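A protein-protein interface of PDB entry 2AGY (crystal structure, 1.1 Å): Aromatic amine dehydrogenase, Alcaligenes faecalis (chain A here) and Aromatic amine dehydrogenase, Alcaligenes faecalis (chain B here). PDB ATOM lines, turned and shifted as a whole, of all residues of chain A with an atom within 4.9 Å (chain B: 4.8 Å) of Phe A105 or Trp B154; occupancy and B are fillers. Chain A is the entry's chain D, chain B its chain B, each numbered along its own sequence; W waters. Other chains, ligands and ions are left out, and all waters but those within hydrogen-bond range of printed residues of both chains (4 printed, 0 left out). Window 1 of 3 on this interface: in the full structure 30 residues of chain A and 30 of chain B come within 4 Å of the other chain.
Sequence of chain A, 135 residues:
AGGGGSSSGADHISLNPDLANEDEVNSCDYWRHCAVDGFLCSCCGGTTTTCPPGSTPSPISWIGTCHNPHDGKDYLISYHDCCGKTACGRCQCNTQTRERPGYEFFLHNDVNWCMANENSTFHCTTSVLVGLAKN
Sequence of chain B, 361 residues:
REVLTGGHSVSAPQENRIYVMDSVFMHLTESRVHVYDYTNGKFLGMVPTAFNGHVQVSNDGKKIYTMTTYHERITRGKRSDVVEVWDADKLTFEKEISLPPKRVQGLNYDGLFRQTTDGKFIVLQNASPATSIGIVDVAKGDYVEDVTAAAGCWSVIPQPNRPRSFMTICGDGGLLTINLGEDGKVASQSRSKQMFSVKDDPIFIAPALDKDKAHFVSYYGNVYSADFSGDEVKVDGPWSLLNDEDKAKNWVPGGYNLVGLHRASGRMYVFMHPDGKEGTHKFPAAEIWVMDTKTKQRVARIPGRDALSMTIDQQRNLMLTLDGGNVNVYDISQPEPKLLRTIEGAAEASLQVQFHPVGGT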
ATOM      1  N   PRO A 101     -10.196 -22.332 -30.082  1.00  0.00           N
ATOM      2  CA  PRO A 101      -9.217 -22.810 -29.110  1.00  0.00           C
ATOM      3  C   PRO A 101      -7.775 -22.713 -29.581  1.00  0.00           C
ATOM      4  O   PRO A 101      -7.496 -22.302 -30.711  1.00  0.00           O
ATOM      5  CB  PRO A 101      -9.618 -24.272 -28.894  1.00  0.00           C
ATOM      6  CG  PRO A 101     -11.024 -24.361 -29.423  1.00  0.00           C
ATOM      7  CD  PRO A 101     -11.039 -23.428 -30.589  1.00  0.00           C
ATOM      8  N   GLY A 102      -6.867 -23.113 -28.690  1.00  0.00           N
ATOM      9  CA  GLY A 102      -5.449 -22.873 -28.873  1.00  0.00           C
ATOM     10  C   GLY A 102      -4.813 -23.603 -30.042  1.00  0.00           C
ATOM     11  O   GLY A 102      -3.715 -23.249 -30.441  1.00  0.00           O
ATOM     12  N   TYR A 103      -5.495 -24.611 -30.595  1.00  0.00           N
ATOM     13  CA  TYR A 103      -5.031 -25.241 -31.829  1.00  0.00           C
ATOM     14  C   TYR A 103      -5.308 -24.383 -33.067  1.00  0.00           C
ATOM     15  O   TYR A 103      -4.855 -24.717 -34.157  1.00  0.00           O
ATOM     16  CB  TYR A 103      -5.605 -26.658 -31.988  1.00  0.00           C
ATOM     17  CG  TYR A 103      -7.104 -26.736 -31.965  1.00  0.00           C
ATOM     18  CD1 TYR A 103      -7.852 -26.340 -33.056  1.00  0.00           C
ATOM     19  CD2 TYR A 103      -7.781 -27.213 -30.846  1.00  0.00           C
ATOM     20  CE1 TYR A 103      -9.221 -26.405 -33.039  1.00  0.00           C
ATOM     21  CE2 TYR A 103      -9.167 -27.283 -30.828  1.00  0.00           C
ATOM     22  CZ  TYR A 103      -9.878 -26.877 -31.929  1.00  0.00           C
ATOM     23  OH  TYR A 103     -11.236 -26.933 -31.940  1.00  0.00           O
ATOM     24  N   GLU A 104      -6.043 -23.286 -32.902  1.00  0.00           N
ATOM     25  CA  GLU A 104      -6.054 -22.170 -33.866  1.00  0.00           C
ATOM     26  C   GLU A 104      -5.566 -20.919 -33.146  1.00  0.00           C
ATOM     27  O   GLU A 104      -6.348 -20.033 -32.802  1.00  0.00           O
ATOM     28  CB  GLU A 104      -7.472 -21.935 -34.415  1.00  0.00           C
ATOM     29  CG  GLU A 104      -8.140 -23.166 -35.010  1.00  0.00           C
ATOM     30  CD  GLU A 104      -9.554 -22.883 -35.501  1.00  0.00           C
ATOM     31  OE1 GLU A 104      -9.702 -22.068 -36.429  1.00  0.00           O
ATOM     32  OE2 GLU A 104     -10.519 -23.490 -34.951  1.00  0.00           O
ATOM     33  N   PHE A 105      -4.267 -20.855 -32.925  1.00  0.00           N
ATOM     34  CA  PHE A 105      -3.741 -20.091 -31.803  1.00  0.00           C
ATOM     35  C   PHE A 105      -4.024 -18.614 -31.914  1.00  0.00           C
ATOM     36  O   PHE A 105      -4.321 -17.978 -30.911  1.00  0.00           O
ATOM     37  CB  PHE A 105      -2.244 -20.341 -31.627  1.00  0.00           C
ATOM     38  CG  PHE A 105      -1.718 -20.017 -30.226  1.00  0.00           C
ATOM     39  CD1 PHE A 105      -2.336 -20.509 -29.097  1.00  0.00           C
ATOM     40  CD2 PHE A 105      -0.604 -19.221 -30.063  1.00  0.00           C
ATOM     41  CE1 PHE A 105      -1.849 -20.210 -27.840  1.00  0.00           C
ATOM     42  CE2 PHE A 105      -0.128 -18.929 -28.797  1.00  0.00           C
ATOM     43  CZ  PHE A 105      -0.755 -19.431 -27.701  1.00  0.00           C
ATOM     44  N   PHE A 106      -3.932 -18.050 -33.116  1.00  0.00           N
ATOM     45  CA  PHE A 106      -4.067 -16.611 -33.236  1.00  0.00           C
ATOM     46  C   PHE A 106      -5.523 -16.155 -33.323  1.00  0.00           C
ATOM     47  O   PHE A 106      -5.793 -14.981 -33.502  1.00  0.00           O
ATOM     48  CB  PHE A 106      -3.194 -16.089 -34.358  1.00  0.00           C
ATOM     49  CG  PHE A 106      -1.746 -16.261 -34.076  1.00  0.00           C
ATOM     50  CD1 PHE A 106      -1.070 -17.395 -34.497  1.00  0.00           C
ATOM     51  CD2 PHE A 106      -1.054 -15.304 -33.355  1.00  0.00           C
ATOM     52  CE1 PHE A 106       0.281 -17.552 -34.213  1.00  0.00           C
ATOM     53  CE2 PHE A 106       0.300 -15.464 -33.074  1.00  0.00           C
ATOM     54  CZ  PHE A 106       0.956 -16.580 -33.500  1.00  0.00           C
ATOM     55  N   LEU A 107      -6.453 -17.103 -33.159  1.00  0.00           N
ATOM     56  CA  LEU A 107      -7.868 -16.792 -32.979  1.00  0.00           C
ATOM     57  C   LEU A 107      -8.308 -16.998 -31.539  1.00  0.00           C
ATOM     58  O   LEU A 107      -9.479 -16.891 -31.252  1.00  0.00           O
ATOM     59  CB  LEU A 107      -8.730 -17.700 -33.881  1.00  0.00           C
ATOM     60  CG  LEU A 107      -8.499 -17.607 -35.368  1.00  0.00           C
ATOM     61  CD1 LEU A 107      -9.496 -18.474 -36.137  1.00  0.00           C
ATOM     62  CD2 LEU A 107      -8.579 -16.186 -35.842  1.00  0.00           C
ATOM     63  N   HIS A 108      -7.358 -17.299 -30.648  1.00  0.00           N
ATOM     64  CA  HIS A 108      -7.643 -17.756 -29.320  1.00  0.00           C
ATOM     65  C   HIS A 108      -7.394 -16.666 -28.280  1.00  0.00           C
ATOM     66  O   HIS A 108      -6.355 -16.032 -28.297  1.00  0.00           O
ATOM     67  CB  HIS A 108      -6.728 -18.944 -29.010  1.00  0.00           C
ATOM     68  CG  HIS A 108      -7.039 -19.593 -27.714  1.00  0.00           C
ATOM     69  ND1 HIS A 108      -6.089 -19.954 -26.778  1.00  0.00           N
ATOM     70  CD2 HIS A 108      -8.229 -19.943 -27.195  1.00  0.00           C
ATOM     71  CE1 HIS A 108      -6.697 -20.503 -25.737  1.00  0.00           C
ATOM     72  NE2 HIS A 108      -7.992 -20.503 -25.968  1.00  0.00           N
ATOM     73  N   VAL A 111      -5.387 -16.927 -23.710  1.00  0.00           N
ATOM     74  CA  VAL A 111      -3.970 -16.805 -23.404  1.00  0.00           C
ATOM     75  C   VAL A 111      -3.605 -15.339 -23.310  1.00  0.00           C
ATOM     76  O   VAL A 111      -4.314 -14.469 -23.813  1.00  0.00           O
ATOM     77  CB  VAL A 111      -3.087 -17.520 -24.444  1.00  0.00           C
ATOM     78  CG1 VAL A 111      -3.268 -19.027 -24.341  1.00  0.00           C
ATOM     79  CG2 VAL A 111      -3.388 -17.021 -25.838  1.00  0.00           C
ATOM     80  N   TRP A 113      -1.769 -12.372 -24.491  1.00  0.00           N
ATOM     81  CA  TRP A 113      -1.058 -11.950 -25.669  1.00  0.00           C
ATOM     82  C   TRP A 113       0.144 -11.044 -25.345  1.00  0.00           C
ATOM     83  O   TRP A 113       0.875 -10.662 -26.245  1.00  0.00           O
ATOM     84  CB  TRP A 113      -2.022 -11.437 -26.793  1.00  0.00           C
ATOM     85  CG  TRP A 113      -2.602 -12.629 -27.481  1.00  0.00           C
ATOM     86  CD1 TRP A 113      -3.905 -13.082 -27.467  1.00  0.00           C
ATOM     87  CD2 TRP A 113      -1.880 -13.554 -28.255  1.00  0.00           C
ATOM     88  NE1 TRP A 113      -4.013 -14.238 -28.191  1.00  0.00           N
ATOM     89  CE2 TRP A 113      -2.776 -14.546 -28.694  1.00  0.00           C
ATOM     90  CE3 TRP A 113      -0.544 -13.643 -28.656  1.00  0.00           C
ATOM     91  CZ2 TRP A 113      -2.381 -15.597 -29.491  1.00  0.00           C
ATOM     92  CZ3 TRP A 113      -0.156 -14.699 -29.454  1.00  0.00           C
ATOM     93  CH2 TRP A 113      -1.067 -15.654 -29.864  1.00  0.00           C
ATOM     94  N   MET A 115       2.497 -12.473 -23.724  1.00  0.00           N
ATOM     95  CA  MET A 115       3.385 -13.589 -23.339  1.00  0.00           C
ATOM     96  C   MET A 115       4.818 -13.449 -23.824  1.00  0.00           C
ATOM     97  O   MET A 115       5.720 -14.053 -23.253  1.00  0.00           O
ATOM     98  CB  MET A 115       2.820 -14.912 -23.866  1.00  0.00           C
ATOM     99  CG  MET A 115       2.801 -15.015 -25.351  1.00  0.00           C
ATOM    100  SD  MET A 115       2.077 -16.563 -25.961  1.00  0.00           S
ATOM    101  CE  MET A 115       0.337 -16.108 -26.066  1.00  0.00           C
ATOM    102  N   VAL B 104       3.132 -21.508 -20.870  1.00  0.00           N
ATOM    103  CA  VAL B 104       1.863 -20.901 -21.264  1.00  0.00           C
ATOM    104  C   VAL B 104       1.307 -20.034 -20.150  1.00  0.00           C
ATOM    105  O   VAL B 104       1.180 -20.479 -18.996  1.00  0.00           O
ATOM    106  CB  VAL B 104       0.801 -21.956 -21.649  1.00  0.00           C
ATOM    107  CG1 VAL B 104       0.489 -22.940 -20.491  1.00  0.00           C
ATOM    108  CG2 VAL B 104      -0.465 -21.273 -22.162  1.00  0.00           C
ATOM    109  N   LEU B 112      -3.068 -27.849 -19.895  1.00  0.00           N
ATOM    110  CA  LEU B 112      -1.883 -27.013 -20.018  1.00  0.00           C
ATOM    111  C   LEU B 112      -0.750 -27.419 -19.068  1.00  0.00           C
ATOM    112  O   LEU B 112       0.381 -26.980 -19.224  1.00  0.00           O
ATOM    113  CB  LEU B 112      -2.261 -25.538 -19.861  1.00  0.00           C
ATOM    114  CG  LEU B 112      -3.283 -25.062 -20.888  1.00  0.00           C
ATOM    115  CD1 LEU B 112      -3.650 -23.639 -20.637  1.00  0.00           C
ATOM    116  CD2 LEU B 112      -2.759 -25.247 -22.318  1.00  0.00           C
ATOM    117  N   GLN B 125       2.450 -27.043 -21.445  1.00  0.00           N
ATOM    118  CA  GLN B 125       2.342 -26.332 -22.706  1.00  0.00           C
ATOM    119  C   GLN B 125       3.199 -25.062 -22.704  1.00  0.00           C
ATOM    120  O   GLN B 125       3.100 -24.267 -21.777  1.00  0.00           O
ATOM    121  CB  GLN B 125       0.876 -25.959 -22.988  1.00  0.00           C
ATOM    122  CG  GLN B 125       0.640 -25.263 -24.298  1.00  0.00           C
ATOM    123  CD  GLN B 125       0.964 -26.147 -25.485  1.00  0.00           C
ATOM    124  OE1 GLN B 125       1.872 -25.840 -26.277  1.00  0.00           O
ATOM    125  NE2 GLN B 125       0.253 -27.227 -25.609  1.00  0.00           N
ATOM    126  N   ASN B 126       4.026 -24.902 -23.737  1.00  0.00           N
ATOM    127  CA  ASN B 126       4.783 -23.683 -23.971  1.00  0.00           C
ATOM    128  C   ASN B 126       4.158 -22.875 -25.104  1.00  0.00           C
ATOM    129  O   ASN B 126       3.551 -23.426 -26.028  1.00  0.00           O
ATOM    130  CB  ASN B 126       6.200 -24.009 -24.436  1.00  0.00           C
ATOM    131  CG  ASN B 126       7.072 -24.599 -23.356  1.00  0.00           C
ATOM    132  OD1 ASN B 126       6.977 -24.241 -22.195  1.00  0.00           O
ATOM    133  ND2 ASN B 126       7.969 -25.512 -23.758  1.00  0.00           N
ATOM    134  N   ALA B 127       4.333 -21.577 -25.036  1.00  0.00           N
ATOM    135  CA  ALA B 127       3.951 -20.700 -26.147  1.00  0.00           C
ATOM    136  C   ALA B 127       4.812 -19.470 -26.126  1.00  0.00           C
ATOM    137  O   ALA B 127       4.854 -18.751 -25.127  1.00  0.00           O
ATOM    138  CB  ALA B 127       2.499 -20.319 -26.041  1.00  0.00           C
ATOM    139  N   PRO B 129       5.280 -16.961 -29.157  1.00  0.00           N
ATOM    140  CA  PRO B 129       4.034 -17.715 -29.143  1.00  0.00           C
ATOM    141  C   PRO B 129       4.083 -19.036 -29.911  1.00  0.00           C
ATOM    142  O   PRO B 129       3.086 -19.737 -29.960  1.00  0.00           O
ATOM    143  CB  PRO B 129       3.058 -16.766 -29.858  1.00  0.00           C
ATOM    144  CG  PRO B 129       3.930 -15.976 -30.797  1.00  0.00           C
ATOM    145  CD  PRO B 129       5.212 -15.801 -30.064  1.00  0.00           C
ATOM    146  N   THR B 131       4.339 -22.770 -30.403  1.00  0.00           N
ATOM    147  CA  THR B 131       4.000 -23.767 -29.402  1.00  0.00           C
ATOM    148  C   THR B 131       4.926 -24.958 -29.423  1.00  0.00           C
ATOM    149  O   THR B 131       5.409 -25.383 -30.447  1.00  0.00           O
ATOM    150  CB  THR B 131       2.487 -24.199 -29.432  1.00  0.00           C
ATOM    151  OG1 THR B 131       2.226 -25.132 -30.489  1.00  0.00           O
ATOM    152  CG2 THR B 131       1.567 -22.984 -29.659  1.00  0.00           C
ATOM    153  N   GLY B 152       2.225 -25.995 -33.524  1.00  0.00           N
ATOM    154  CA  GLY B 152       0.908 -25.890 -34.143  1.00  0.00           C
ATOM    155  C   GLY B 152      -0.149 -26.760 -33.476  1.00  0.00           C
ATOM    156  O   GLY B 152      -1.267 -26.876 -33.989  1.00  0.00           O
ATOM    157  N   CYS B 153       0.206 -27.371 -32.340  1.00  0.00           N
ATOM    158  CA  CYS B 153      -0.736 -28.163 -31.559  1.00  0.00           C
ATOM    159  C   CYS B 153      -0.992 -27.456 -30.248  1.00  0.00           C
ATOM    160  O   CYS B 153      -0.372 -26.431 -29.954  1.00  0.00           O
ATOM    161  CB  CYS B 153      -0.194 -29.558 -31.299  1.00  0.00           C
ATOM    162  SG  CYS B 153       0.337 -30.414 -32.792  1.00  0.00           S
ATOM    163  N   TRP B 154      -1.914 -28.005 -29.452  1.00  0.00           N
ATOM    164  CA  TRP B 154      -2.278 -27.384 -28.183  1.00  0.00           C
ATOM    165  C   TRP B 154      -2.815 -28.386 -27.205  1.00  0.00           C
ATOM    166  O   TRP B 154      -3.702 -29.170 -27.527  1.00  0.00           O
ATOM    167  CB  TRP B 154      -3.311 -26.298 -28.405  1.00  0.00           C
ATOM    168  CG  TRP B 154      -3.465 -25.351 -27.281  1.00  0.00           C
ATOM    169  CD1 TRP B 154      -4.559 -25.191 -26.496  1.00  0.00           C
ATOM    170  CD2 TRP B 154      -2.501 -24.404 -26.829  1.00  0.00           C
ATOM    171  NE1 TRP B 154      -4.329 -24.210 -25.567  1.00  0.00           N
ATOM    172  CE2 TRP B 154      -3.068 -23.708 -25.754  1.00  0.00           C
ATOM    173  CE3 TRP B 154      -1.201 -24.082 -27.223  1.00  0.00           C
ATOM    174  CZ2 TRP B 154      -2.394 -22.717 -25.082  1.00  0.00           C
ATOM    175  CZ3 TRP B 154      -0.531 -23.103 -26.561  1.00  0.00           C
ATOM    176  CH2 TRP B 154      -1.129 -22.427 -25.486  1.00  0.00           C
ATOM    177  N   SER B 155      -2.253 -28.323 -26.005  1.00  0.00           N
ATOM    178  CA  SER B 155      -2.707 -29.008 -24.810  1.00  0.00           C
ATOM    179  C   SER B 155      -2.257 -30.454 -24.747  1.00  0.00           C
ATOM    180  O   SER B 155      -1.881 -31.039 -25.765  1.00  0.00           O
ATOM    181  CB  SER B 155      -4.228 -28.867 -24.607  1.00  0.00           C
ATOM    182  OG  SER B 155      -4.953 -29.890 -25.263  1.00  0.00           O
ATOM    183  N   VAL B 156      -2.296 -31.014 -23.544  1.00  0.00           N
ATOM    184  CA  VAL B 156      -1.688 -32.287 -23.235  1.00  0.00           C
ATOM    185  C   VAL B 156      -2.766 -33.209 -22.690  1.00  0.00           C
ATOM    186  O   VAL B 156      -3.407 -32.899 -21.692  1.00  0.00           O
ATOM    187  CB  VAL B 156      -0.589 -32.129 -22.156  1.00  0.00           C
ATOM    188  CG1 VAL B 156       0.004 -33.453 -21.786  1.00  0.00           C
ATOM    189  CG2 VAL B 156       0.504 -31.167 -22.657  1.00  0.00           C
ATOM    190  N   THR B 168      -1.645 -34.582 -28.114  1.00  0.00           N
ATOM    191  CA  THR B 168      -1.999 -33.200 -28.205  1.00  0.00           C
ATOM    192  C   THR B 168      -2.878 -32.995 -29.437  1.00  0.00           C
ATOM    193  O   THR B 168      -2.842 -33.810 -30.363  1.00  0.00           O
ATOM    194  CB  THR B 168      -0.729 -32.331 -28.209  1.00  0.00           C
ATOM    195  OG1 THR B 168      -1.090 -30.949 -28.273  1.00  0.00           O
ATOM    196  CG2 THR B 168       0.137 -32.589 -29.433  1.00  0.00           C
ATOM    197  N   ILE B 169      -3.665 -31.927 -29.445  1.00  0.00           N
ATOM    198  CA  ILE B 169      -4.602 -31.644 -30.518  1.00  0.00           C
ATOM    199  C   ILE B 169      -3.952 -30.693 -31.476  1.00  0.00           C
ATOM    200  O   ILE B 169      -3.474 -29.646 -31.082  1.00  0.00           O
ATOM    201  CB  ILE B 169      -5.892 -30.987 -29.977  1.00  0.00           C
ATOM    202  CG1 ILE B 169      -6.568 -31.871 -28.938  1.00  0.00           C
ATOM    203  CG2 ILE B 169      -6.839 -30.693 -31.112  1.00  0.00           C
ATOM    204  CD1 ILE B 169      -7.593 -31.133 -28.076  1.00  0.00           C
ATOM    205  N   ILE B 205     -11.103 -28.310 -26.158  1.00  0.00           N
ATOM    206  CA  ILE B 205      -9.898 -29.085 -25.897  1.00  0.00           C
ATOM    207  C   ILE B 205     -10.030 -30.044 -24.724  1.00  0.00           C
ATOM    208  O   ILE B 205      -9.275 -30.999 -24.621  1.00  0.00           O
ATOM    209  CB  ILE B 205      -8.651 -28.165 -25.720  1.00  0.00           C
ATOM    210  CG1 ILE B 205      -8.790 -27.273 -24.475  1.00  0.00           C
ATOM    211  CG2 ILE B 205      -8.409 -27.349 -26.977  1.00  0.00           C
ATOM    212  CD1 ILE B 205      -7.478 -26.726 -23.973  1.00  0.00           C
HETATM  213  O   HOH W   1      -1.303 -24.164 -31.477  1.00  0.00           O
HETATM  214  O   HOH W   2      -7.740 -23.816 -25.999  1.00  0.00           O
HETATM  215  O   HOH W   3      -6.009 -22.557 -23.988  1.00  0.00           O
HETATM  216  O   HOH W   4      -2.440 -24.817 -35.429  1.00  0.00           O
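The backbone carbonyl oxygen (O) of Trp B154 lies within hydrogen-bond range of the side-chain hydroxyl (OG1) of Thr B168, 3.2 Å away.
NE1 of Trp A113 is in hydrogen-bond range of O of His A108, 3.0 Å away.
O of Ile B169 is in hydrogen-bond range of N of Trp B154.
Among the printed residues, merely in contact across the chains: Phe A105 with Trp B154, Gly A102 with Trp B154, Phe A105 with Pro B129, Tyr A103 with Trp B154, Tyr A103 with Ile B169, Phe A105 with Ala B127, Pro A101 with Ile B205, Trp A113 with Pro B129, Val A111 with Trp B154, Met A115 with Pro B129 and Tyr A103 with Ile B205.
Of the 11 printed residues of chain A, 7 touch a printed residue of chain B.
Of the 15 printed residues of chain B, 5 touch a printed residue of chain A.
Among the printed residues, 12 pairs touch across the chains.
Among the printed residues, no Asp or Glu carboxylate lies within 4 Å of a Lys or Arg side-chain nitrogen of the other chain.
Phe A105 touches three residues of chain B.
Of chain A, only Gly A102 (3.4 Å), Tyr A103 (3.5 Å), Phe A105 (3.3 Å) and Val A111 (3.9 Å) come within 4 Å of Trp B154.
Of the printed residues of chain A, Ala B127 touches Phe A105 (3.8 Å) and Met A115 (3.6 Å).
Printed residues of chain B within 4 Å of Met A115: Ala B127 (3.6 Å) and Pro B129 (3.9 Å).
Printed residues of chain B within 4 Å of Val A111: Trp B154.
Of the printed residues of chain A, Pro B129 touches Phe A105, Trp A113 and Met A115.
The nearest printed residue of chain A that does not touch Ile B169 is Gly A102 (6.3 Å).
Water W4 lies within hydrogen-bond range of O of Tyr A103 and O of Gly B152.
Water W1 bridges O of Gly A102 and O of Cys B153.
Water W3 lies within hydrogen-bond range of the indole nitrogen (NE1) of Trp B154 and a ring nitrogen (NE2) of His A108.
Water W2 lies within hydrogen-bond range of the backbone NH of Gly A102 (2.9 Å), a ring nitrogen (NE2) of His A108 (3.3 Å) and the indole nitrogen of Trp B154 (3.5 Å).
The side-chain sulfur (SD) of Met A115 lies close to the backbone carbonyl oxygen (O) of Ala B127.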
